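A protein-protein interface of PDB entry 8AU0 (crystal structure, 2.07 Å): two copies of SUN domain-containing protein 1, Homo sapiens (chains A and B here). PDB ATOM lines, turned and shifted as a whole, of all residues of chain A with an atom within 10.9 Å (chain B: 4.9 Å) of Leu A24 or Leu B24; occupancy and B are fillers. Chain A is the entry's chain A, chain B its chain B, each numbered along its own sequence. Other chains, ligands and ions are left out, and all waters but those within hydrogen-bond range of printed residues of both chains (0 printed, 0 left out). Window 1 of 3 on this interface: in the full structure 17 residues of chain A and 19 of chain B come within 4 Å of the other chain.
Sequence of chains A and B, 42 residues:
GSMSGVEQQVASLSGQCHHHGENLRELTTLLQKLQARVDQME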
ATOM      1  N   GLY A  15      -5.190   9.338  19.049  1.00  0.00           N
ATOM      2  CA  GLY A  15      -4.715  10.337  18.106  1.00  0.00           C
ATOM      3  C   GLY A  15      -5.415  10.247  16.763  1.00  0.00           C
ATOM      4  O   GLY A  15      -5.779  11.268  16.172  1.00  0.00           O
ATOM      5  N   GLN A  16      -5.609   9.023  16.261  1.00  0.00           N
ATOM      6  CA  GLN A  16      -6.355   8.838  15.018  1.00  0.00           C
ATOM      7  C   GLN A  16      -7.800   9.291  15.176  1.00  0.00           C
ATOM      8  O   GLN A  16      -8.381   9.882  14.257  1.00  0.00           O
ATOM      9  CB  GLN A  16      -6.308   7.371  14.588  1.00  0.00           C
ATOM     10  CG  GLN A  16      -4.952   6.873  14.136  1.00  0.00           C
ATOM     11  CD  GLN A  16      -4.945   5.374  13.907  1.00  0.00           C
ATOM     12  OE1 GLN A  16      -5.567   4.615  14.653  1.00  0.00           O
ATOM     13  NE2 GLN A  16      -4.249   4.938  12.865  1.00  0.00           N
ATOM     14  N   CYS A  17      -8.396   9.002  16.335  1.00  0.00           N
ATOM     15  CA  CYS A  17      -9.742   9.473  16.641  1.00  0.00           C
ATOM     16  C   CYS A  17      -9.833  10.990  16.518  1.00  0.00           C
ATOM     17  O   CYS A  17     -10.704  11.515  15.817  1.00  0.00           O
ATOM     18  CB  CYS A  17     -10.130   9.011  18.046  1.00  0.00           C
ATOM     19  SG  CYS A  17     -11.761   9.513  18.607  1.00  0.00           S
ATOM     20  N   HIS A  18      -8.929  11.712  17.191  1.00  0.00           N
ATOM     21  CA  HIS A  18      -8.947  13.172  17.128  1.00  0.00           C
ATOM     22  C   HIS A  18      -8.725  13.671  15.706  1.00  0.00           C
ATOM     23  O   HIS A  18      -9.346  14.652  15.282  1.00  0.00           O
ATOM     24  CB  HIS A  18      -7.889  13.763  18.060  1.00  0.00           C
ATOM     25  CG  HIS A  18      -7.777  15.254  17.970  1.00  0.00           C
ATOM     26  ND1 HIS A  18      -6.853  15.883  17.163  1.00  0.00           N
ATOM     27  CD2 HIS A  18      -8.481  16.241  18.575  1.00  0.00           C
ATOM     28  CE1 HIS A  18      -6.988  17.192  17.281  1.00  0.00           C
ATOM     29  NE2 HIS A  18      -7.969  17.435  18.131  1.00  0.00           N
ATOM     30  N   HIS A  19      -7.834  13.012  14.959  1.00  0.00           N
ATOM     31  CA  HIS A  19      -7.621  13.377  13.562  1.00  0.00           C
ATOM     32  C   HIS A  19      -8.896  13.192  12.748  1.00  0.00           C
ATOM     33  O   HIS A  19      -9.273  14.074  11.966  1.00  0.00           O
ATOM     34  CB  HIS A  19      -6.477  12.549  12.977  1.00  0.00           C
ATOM     35  CG  HIS A  19      -6.033  12.992  11.617  1.00  0.00           C
ATOM     36  ND1 HIS A  19      -5.804  12.106  10.587  1.00  0.00           N
ATOM     37  CD2 HIS A  19      -5.765  14.223  11.121  1.00  0.00           C
ATOM     38  CE1 HIS A  19      -5.417  12.772   9.513  1.00  0.00           C
ATOM     39  NE2 HIS A  19      -5.386  14.058   9.810  1.00  0.00           N
ATOM     40  N   HIS A  20      -9.576  12.055  12.926  1.00  0.00           N
ATOM     41  CA  HIS A  20     -10.864  11.843  12.272  1.00  0.00           C
ATOM     42  C   HIS A  20     -11.861  12.931  12.648  1.00  0.00           C
ATOM     43  O   HIS A  20     -12.625  13.401  11.798  1.00  0.00           O
ATOM     44  CB  HIS A  20     -11.429  10.469  12.637  1.00  0.00           C
ATOM     45  CG  HIS A  20     -10.742   9.327  11.957  1.00  0.00           C
ATOM     46  ND1 HIS A  20      -9.779   9.508  10.991  1.00  0.00           N
ATOM     47  CD2 HIS A  20     -10.890   7.989  12.101  1.00  0.00           C
ATOM     48  CE1 HIS A  20      -9.357   8.327  10.569  1.00  0.00           C
ATOM     49  NE2 HIS A  20     -10.015   7.390  11.227  1.00  0.00           N
ATOM     50  N   GLY A  21     -11.875  13.337  13.919  1.00  0.00           N
ATOM     51  CA  GLY A  21     -12.765  14.412  14.332  1.00  0.00           C
ATOM     52  C   GLY A  21     -12.439  15.728  13.664  1.00  0.00           C
ATOM     53  O   GLY A  21     -13.336  16.520  13.349  1.00  0.00           O
ATOM     54  N   GLU A  22     -11.149  15.989  13.426  1.00  0.00           N
ATOM     55  CA  GLU A  22     -10.747  17.184  12.701  1.00  0.00           C
ATOM     56  C   GLU A  22     -11.222  17.131  11.253  1.00  0.00           C
ATOM     57  O   GLU A  22     -11.733  18.120  10.718  1.00  0.00           O
ATOM     58  CB  GLU A  22      -9.228  17.354  12.760  1.00  0.00           C
ATOM     59  CG  GLU A  22      -8.679  17.590  14.157  1.00  0.00           C
ATOM     60  CD  GLU A  22      -9.265  18.825  14.808  1.00  0.00           C
ATOM     61  OE1 GLU A  22      -9.200  19.909  14.191  1.00  0.00           O
ATOM     62  OE2 GLU A  22      -9.799  18.706  15.931  1.00  0.00           O
ATOM     63  N   ASN A  23     -11.051  15.975  10.602  1.00  0.00           N
ATOM     64  CA  ASN A  23     -11.491  15.834   9.217  1.00  0.00           C
ATOM     65  C   ASN A  23     -13.001  16.004   9.096  1.00  0.00           C
ATOM     66  O   ASN A  23     -13.489  16.614   8.137  1.00  0.00           O
ATOM     67  CB  ASN A  23     -11.057  14.475   8.662  1.00  0.00           C
ATOM     68  CG  ASN A  23      -9.562  14.392   8.420  1.00  0.00           C
ATOM     69  OD1 ASN A  23      -8.895  15.410   8.254  1.00  0.00           O
ATOM     70  ND2 ASN A  23      -9.031  13.174   8.395  1.00  0.00           N
ATOM     71  N   LEU A  24     -13.755  15.476  10.065  1.00  0.00           N
ATOM     72  CA  LEU A  24     -15.207  15.619  10.035  1.00  0.00           C
ATOM     73  C   LEU A  24     -15.613  17.085  10.106  1.00  0.00           C
ATOM     74  O   LEU A  24     -16.490  17.531   9.356  1.00  0.00           O
ATOM     75  CB  LEU A  24     -15.837  14.818  11.178  1.00  0.00           C
ATOM     76  CG  LEU A  24     -15.958  13.304  10.975  1.00  0.00           C
ATOM     77  CD1 LEU A  24     -16.210  12.583  12.294  1.00  0.00           C
ATOM     78  CD2 LEU A  24     -17.062  12.987   9.976  1.00  0.00           C
ATOM     79  N   ARG A  25     -14.970  17.856  10.987  1.00  0.00           N
ATOM     80  CA  ARG A  25     -15.294  19.274  11.105  1.00  0.00           C
ATOM     81  C   ARG A  25     -14.946  20.034   9.830  1.00  0.00           C
ATOM     82  O   ARG A  25     -15.689  20.927   9.407  1.00  0.00           O
ATOM     83  CB  ARG A  25     -14.561  19.877  12.302  1.00  0.00           C
ATOM     84  CG  ARG A  25     -14.815  21.359  12.477  1.00  0.00           C
ATOM     85  CD  ARG A  25     -13.650  22.044  13.157  1.00  0.00           C
ATOM     86  NE  ARG A  25     -13.272  21.386  14.400  1.00  0.00           N
ATOM     87  CZ  ARG A  25     -12.037  20.985  14.678  1.00  0.00           C
ATOM     88  NH1 ARG A  25     -11.062  21.194  13.803  1.00  0.00           N
ATOM     89  NH2 ARG A  25     -11.776  20.389  15.833  1.00  0.00           N
ATOM     90  N   GLU A  26     -13.817  19.695   9.202  1.00  0.00           N
ATOM     91  CA  GLU A  26     -13.441  20.352   7.955  1.00  0.00           C
ATOM     92  C   GLU A  26     -14.427  20.015   6.841  1.00  0.00           C
ATOM     93  O   GLU A  26     -14.848  20.892   6.078  1.00  0.00           O
ATOM     94  CB  GLU A  26     -12.020  19.953   7.558  1.00  0.00           C
ATOM     95  CG  GLU A  26     -11.618  20.423   6.170  1.00  0.00           C
ATOM     96  CD  GLU A  26     -10.154  20.169   5.866  1.00  0.00           C
ATOM     97  OE1 GLU A  26      -9.359  20.065   6.824  1.00  0.00           O
ATOM     98  OE2 GLU A  26      -9.801  20.077   4.670  1.00  0.00           O
ATOM     99  N   LEU A  27     -14.802  18.738   6.733  1.00  0.00           N
ATOM    100  CA  LEU A  27     -15.777  18.333   5.729  1.00  0.00           C
ATOM    101  C   LEU A  27     -17.130  18.980   5.984  1.00  0.00           C
ATOM    102  O   LEU A  27     -17.866  19.295   5.041  1.00  0.00           O
ATOM    103  CB  LEU A  27     -15.911  16.814   5.715  1.00  0.00           C
ATOM    104  CG  LEU A  27     -15.147  16.076   4.620  1.00  0.00           C
ATOM    105  CD1 LEU A  27     -15.778  16.346   3.265  1.00  0.00           C
ATOM    106  CD2 LEU A  27     -13.684  16.477   4.627  1.00  0.00           C
ATOM    107  N   THR A  28     -17.483  19.175   7.257  1.00  0.00           N
ATOM    108  CA  THR A  28     -18.753  19.819   7.571  1.00  0.00           C
ATOM    109  C   THR A  28     -18.750  21.276   7.130  1.00  0.00           C
ATOM    110  O   THR A  28     -19.746  21.769   6.588  1.00  0.00           O
ATOM    111  CB  THR A  28     -19.045  19.708   9.068  1.00  0.00           C
ATOM    112  OG1 THR A  28     -19.073  18.327   9.453  1.00  0.00           O
ATOM    113  CG2 THR A  28     -20.384  20.344   9.404  1.00  0.00           C
ATOM    114  N   THR A  29     -17.634  21.980   7.339  1.00  0.00           N
ATOM    115  CA  THR A  29     -17.579  23.385   6.951  1.00  0.00           C
ATOM    116  C   THR A  29     -17.596  23.540   5.434  1.00  0.00           C
ATOM    117  O   THR A  29     -18.229  24.462   4.906  1.00  0.00           O
ATOM    118  CB  THR A  29     -16.342  24.055   7.550  1.00  0.00           C
ATOM    119  OG1 THR A  29     -16.314  23.820   8.963  1.00  0.00           O
ATOM    120  CG2 THR A  29     -16.375  25.557   7.300  1.00  0.00           C
ATOM    121  N   LEU A  30     -16.915  22.643   4.716  1.00  0.00           N
ATOM    122  CA  LEU A  30     -16.939  22.711   3.258  1.00  0.00           C
ATOM    123  C   LEU A  30     -18.325  22.387   2.714  1.00  0.00           C
ATOM    124  O   LEU A  30     -18.748  22.959   1.703  1.00  0.00           O
ATOM    125  CB  LEU A  30     -15.896  21.765   2.663  1.00  0.00           C
ATOM    126  CG  LEU A  30     -14.424  22.061   2.941  1.00  0.00           C
ATOM    127  CD1 LEU A  30     -13.522  21.187   2.078  1.00  0.00           C
ATOM    128  CD2 LEU A  30     -14.115  23.533   2.719  1.00  0.00           C
ATOM    129  N   LEU A  31     -19.040  21.467   3.365  1.00  0.00           N
ATOM    130  CA  LEU A  31     -20.397  21.137   2.937  1.00  0.00           C
ATOM    131  C   LEU A  31     -21.333  22.326   3.114  1.00  0.00           C
ATOM    132  O   LEU A  31     -22.187  22.586   2.258  1.00  0.00           O
ATOM    133  CB  LEU A  31     -20.901  19.921   3.716  1.00  0.00           C
ATOM    134  CG  LEU A  31     -22.339  19.450   3.486  1.00  0.00           C
ATOM    135  CD1 LEU A  31     -22.559  18.992   2.053  1.00  0.00           C
ATOM    136  CD2 LEU A  31     -22.667  18.334   4.456  1.00  0.00           C
ATOM    137  N   GLN A  32     -21.175  23.069   4.213  1.00  0.00           N
ATOM    138  CA  GLN A  32     -22.021  24.235   4.454  1.00  0.00           C
ATOM    139  C   GLN A  32     -21.744  25.342   3.447  1.00  0.00           C
ATOM    140  O   GLN A  32     -22.658  26.076   3.050  1.00  0.00           O
ATOM    141  CB  GLN A  32     -21.809  24.756   5.874  1.00  0.00           C
ATOM    142  CG  GLN A  32     -22.218  23.791   6.969  1.00  0.00           C
ATOM    143  CD  GLN A  32     -21.745  24.248   8.333  1.00  0.00           C
ATOM    144  OE1 GLN A  32     -21.009  25.229   8.449  1.00  0.00           O
ATOM    145  NE2 GLN A  32     -22.164  23.541   9.375  1.00  0.00           N
ATOM    146  N   HIS B  20     -13.493   4.104   9.335  1.00  0.00           N
ATOM    147  CA  HIS B  20     -13.897   5.512   9.397  1.00  0.00           C
ATOM    148  C   HIS B  20     -13.026   6.382   8.503  1.00  0.00           C
ATOM    149  O   HIS B  20     -13.512   7.307   7.856  1.00  0.00           O
ATOM    150  CB  HIS B  20     -13.819   6.029  10.835  1.00  0.00           C
ATOM    151  CG  HIS B  20     -14.997   5.686  11.699  1.00  0.00           C
ATOM    152  ND1 HIS B  20     -16.106   5.000  11.236  1.00  0.00           N
ATOM    153  CD2 HIS B  20     -15.245   5.957  13.006  1.00  0.00           C
ATOM    154  CE1 HIS B  20     -16.972   4.853  12.223  1.00  0.00           C
ATOM    155  NE2 HIS B  20     -16.472   5.421  13.311  1.00  0.00           N
ATOM    156  N   GLY B  21     -11.724   6.127   8.481  1.00  0.00           N
ATOM    157  CA  GLY B  21     -10.869   6.872   7.586  1.00  0.00           C
ATOM    158  C   GLY B  21     -11.252   6.668   6.136  1.00  0.00           C
ATOM    159  O   GLY B  21     -11.292   7.619   5.354  1.00  0.00           O
ATOM    160  N   GLU B  22     -11.559   5.430   5.761  1.00  0.00           N
ATOM    161  CA  GLU B  22     -11.919   5.175   4.378  1.00  0.00           C
ATOM    162  C   GLU B  22     -13.247   5.809   4.033  1.00  0.00           C
ATOM    163  O   GLU B  22     -13.450   6.205   2.887  1.00  0.00           O
ATOM    164  CB  GLU B  22     -11.973   3.671   4.090  1.00  0.00           C
ATOM    165  CG  GLU B  22     -10.595   3.002   4.071  1.00  0.00           C
ATOM    166  CD  GLU B  22     -10.649   1.512   3.748  1.00  0.00           C
ATOM    167  OE1 GLU B  22     -11.571   0.825   4.251  1.00  0.00           O
ATOM    168  OE2 GLU B  22      -9.757   1.025   3.005  1.00  0.00           O
ATOM    169  N   ASN B  23     -14.165   5.921   5.001  1.00  0.00           N
ATOM    170  CA  ASN B  23     -15.413   6.636   4.717  1.00  0.00           C
ATOM    171  C   ASN B  23     -15.183   8.139   4.594  1.00  0.00           C
ATOM    172  O   ASN B  23     -15.823   8.789   3.768  1.00  0.00           O
ATOM    173  CB  ASN B  23     -16.474   6.360   5.787  1.00  0.00           C
ATOM    174  CG  ASN B  23     -16.859   4.882   5.881  1.00  0.00           C
ATOM    175  OD1 ASN B  23     -16.980   4.181   4.876  1.00  0.00           O
ATOM    176  ND2 ASN B  23     -17.048   4.411   7.102  1.00  0.00           N
ATOM    177  N   LEU B  24     -14.260   8.696   5.375  1.00  0.00           N
ATOM    178  CA  LEU B  24     -13.896  10.110   5.240  1.00  0.00           C
ATOM    179  C   LEU B  24     -13.319  10.418   3.866  1.00  0.00           C
ATOM    180  O   LEU B  24     -13.732  11.388   3.216  1.00  0.00           O
ATOM    181  CB  LEU B  24     -12.894  10.498   6.342  1.00  0.00           C
ATOM    182  CG  LEU B  24     -13.421  10.674   7.784  1.00  0.00           C
ATOM    183  CD1 LEU B  24     -12.353  10.555   8.869  1.00  0.00           C
ATOM    184  CD2 LEU B  24     -14.125  12.011   7.871  1.00  0.00           C
ATOM    185  N   ARG B  25     -12.357   9.614   3.410  1.00  0.00           N
ATOM    186  CA  ARG B  25     -11.803   9.769   2.065  1.00  0.00           C
ATOM    187  C   ARG B  25     -12.897   9.669   1.000  1.00  0.00           C
ATOM    188  O   ARG B  25     -12.971  10.503   0.087  1.00  0.00           O
ATOM    189  CB  ARG B  25     -10.692   8.724   1.829  1.00  0.00           C
ATOM    190  CG  ARG B  25      -9.374   8.973   2.617  1.00  0.00           C
ATOM    191  CD  ARG B  25      -8.859  10.395   2.369  1.00  0.00           C
ATOM    192  NE  ARG B  25      -7.548  10.716   2.948  1.00  0.00           N
ATOM    193  CZ  ARG B  25      -7.018  11.944   2.924  1.00  0.00           C
ATOM    194  NH1 ARG B  25      -7.694  12.950   2.360  1.00  0.00           N
ATOM    195  NH2 ARG B  25      -5.826  12.178   3.463  1.00  0.00           N
ATOM    196  N   GLU B  26     -13.778   8.671   1.116  1.00  0.00           N
ATOM    197  CA  GLU B  26     -14.912   8.562   0.206  1.00  0.00           C
ATOM    198  C   GLU B  26     -15.731   9.849   0.183  1.00  0.00           C
ATOM    199  O   GLU B  26     -16.045  10.381  -0.878  1.00  0.00           O
ATOM    200  CB  GLU B  26     -15.787   7.377   0.607  1.00  0.00           C
ATOM    201  CG  GLU B  26     -17.064   7.180  -0.237  1.00  0.00           C
ATOM    202  CD  GLU B  26     -18.243   6.474   0.493  1.00  0.00           C
ATOM    203  OE1 GLU B  26     -18.024   5.753   1.501  1.00  0.00           O
ATOM    204  OE2 GLU B  26     -19.407   6.645   0.038  1.00  0.00           O
ATOM    205  N   LEU B  27     -16.095  10.372   1.347  1.00  0.00           N
ATOM    206  CA  LEU B  27     -16.930  11.574   1.353  1.00  0.00           C
ATOM    207  C   LEU B  27     -16.170  12.787   0.837  1.00  0.00           C
ATOM    208  O   LEU B  27     -16.764  13.665   0.210  1.00  0.00           O
ATOM    209  CB  LEU B  27     -17.434  11.868   2.757  1.00  0.00           C
ATOM    210  CG  LEU B  27     -18.462  10.982   3.421  1.00  0.00           C
ATOM    211  CD1 LEU B  27     -18.798  11.655   4.746  1.00  0.00           C
ATOM    212  CD2 LEU B  27     -19.678  10.813   2.526  1.00  0.00           C
ATOM    213  N   THR B  28     -14.872  12.895   1.156  1.00  0.00           N
ATOM    214  CA  THR B  28     -14.094  14.019   0.650  1.00  0.00           C
ATOM    215  C   THR B  28     -14.169  14.045  -0.868  1.00  0.00           C
ATOM    216  O   THR B  28     -14.289  15.112  -1.479  1.00  0.00           O
ATOM    217  CB  THR B  28     -12.632  13.939   1.150  1.00  0.00           C
ATOM    218  OG1 THR B  28     -12.589  13.940   2.576  1.00  0.00           O
ATOM    219  CG2 THR B  28     -11.787  15.130   0.681  1.00  0.00           C
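The backbone NH of Gly B21 sits at hydrogen-bond distance from a ring nitrogen (NE2) of His A20 (3.5 Å).
The side-chain hydroxyl (OG1) of Thr A28 sits at hydrogen-bond distance from the backbone carbonyl oxygen (O) of Leu A24, 2.7 Å away. OG1 of Thr B28 lies within hydrogen-bond range of O of Leu B24 (2.9 Å).
Among the printed residues, pairs that only touch across the chains: Leu A27 with Thr B28 (3.4 Å), His A20 with Leu B24 (3.5 Å), Leu A24 with Leu B24 (3.7 Å) and His A20 with His B20 (3.7 Å).
Of chain B, only Leu B24 (3.7 Å) comes within 4 Å of Leu A24. Of the printed residues of chain A, Leu B24 touches His A20 (3.5 Å) and Leu A24 (3.7 Å). Of chain A, only His A20 (3.5 Å) comes within 4 Å of Gly B21. No residue of chain A comes within 4 Å of Leu B27. Printed residues of chain A within 4 Å of His B20: His A20. Printed residues of chain B within 4 Å of His A20: His B20 (3.7 Å), Gly B21 (3.5 Å) and Leu B24 (3.5 Å). Of the printed residues of chain B, Leu A27 touches Thr B28. Gly A21 touches none of the printed residues of chain B. Gln A32 touches none of the printed residues of chain B. The nearest printed residue of chain B that does not touch His A20 is Glu B22 (6.0 Å).
Printed residues of chain B that touch a printed residue of chain A: His B20, Gly B21, Leu B24 and Thr B28. Hydrophobic or aromatic side chains of chain B within 4 Å of the printed part of chain A: His B20 and Leu B24. Along chain B the printed residues that touch a printed residue of chain A span positions 20 to 28. Among the printed residues, 5 pairs touch across the chains. Among the printed residues, no Asp or Glu carboxylate lies within 4 Å of a Lys or Arg side-chain nitrogen of the other chain.
His B20 touches its own counterpart, His A20. His A20 touches Gly B21, but with the chains exchanged Gly A21 does not touch His B20 (8.2 Å). Leu B24 touches its own counterpart, Leu A24. Leu A27 touches Thr B28, but with the chains exchanged Thr A28 does not touch Leu B27 (8.0 Å). 9 positions are printed for both chains. Of the 5 pairs that touch across the chains among the printed residues, 2 have their exchanged pair printed and touching as well.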
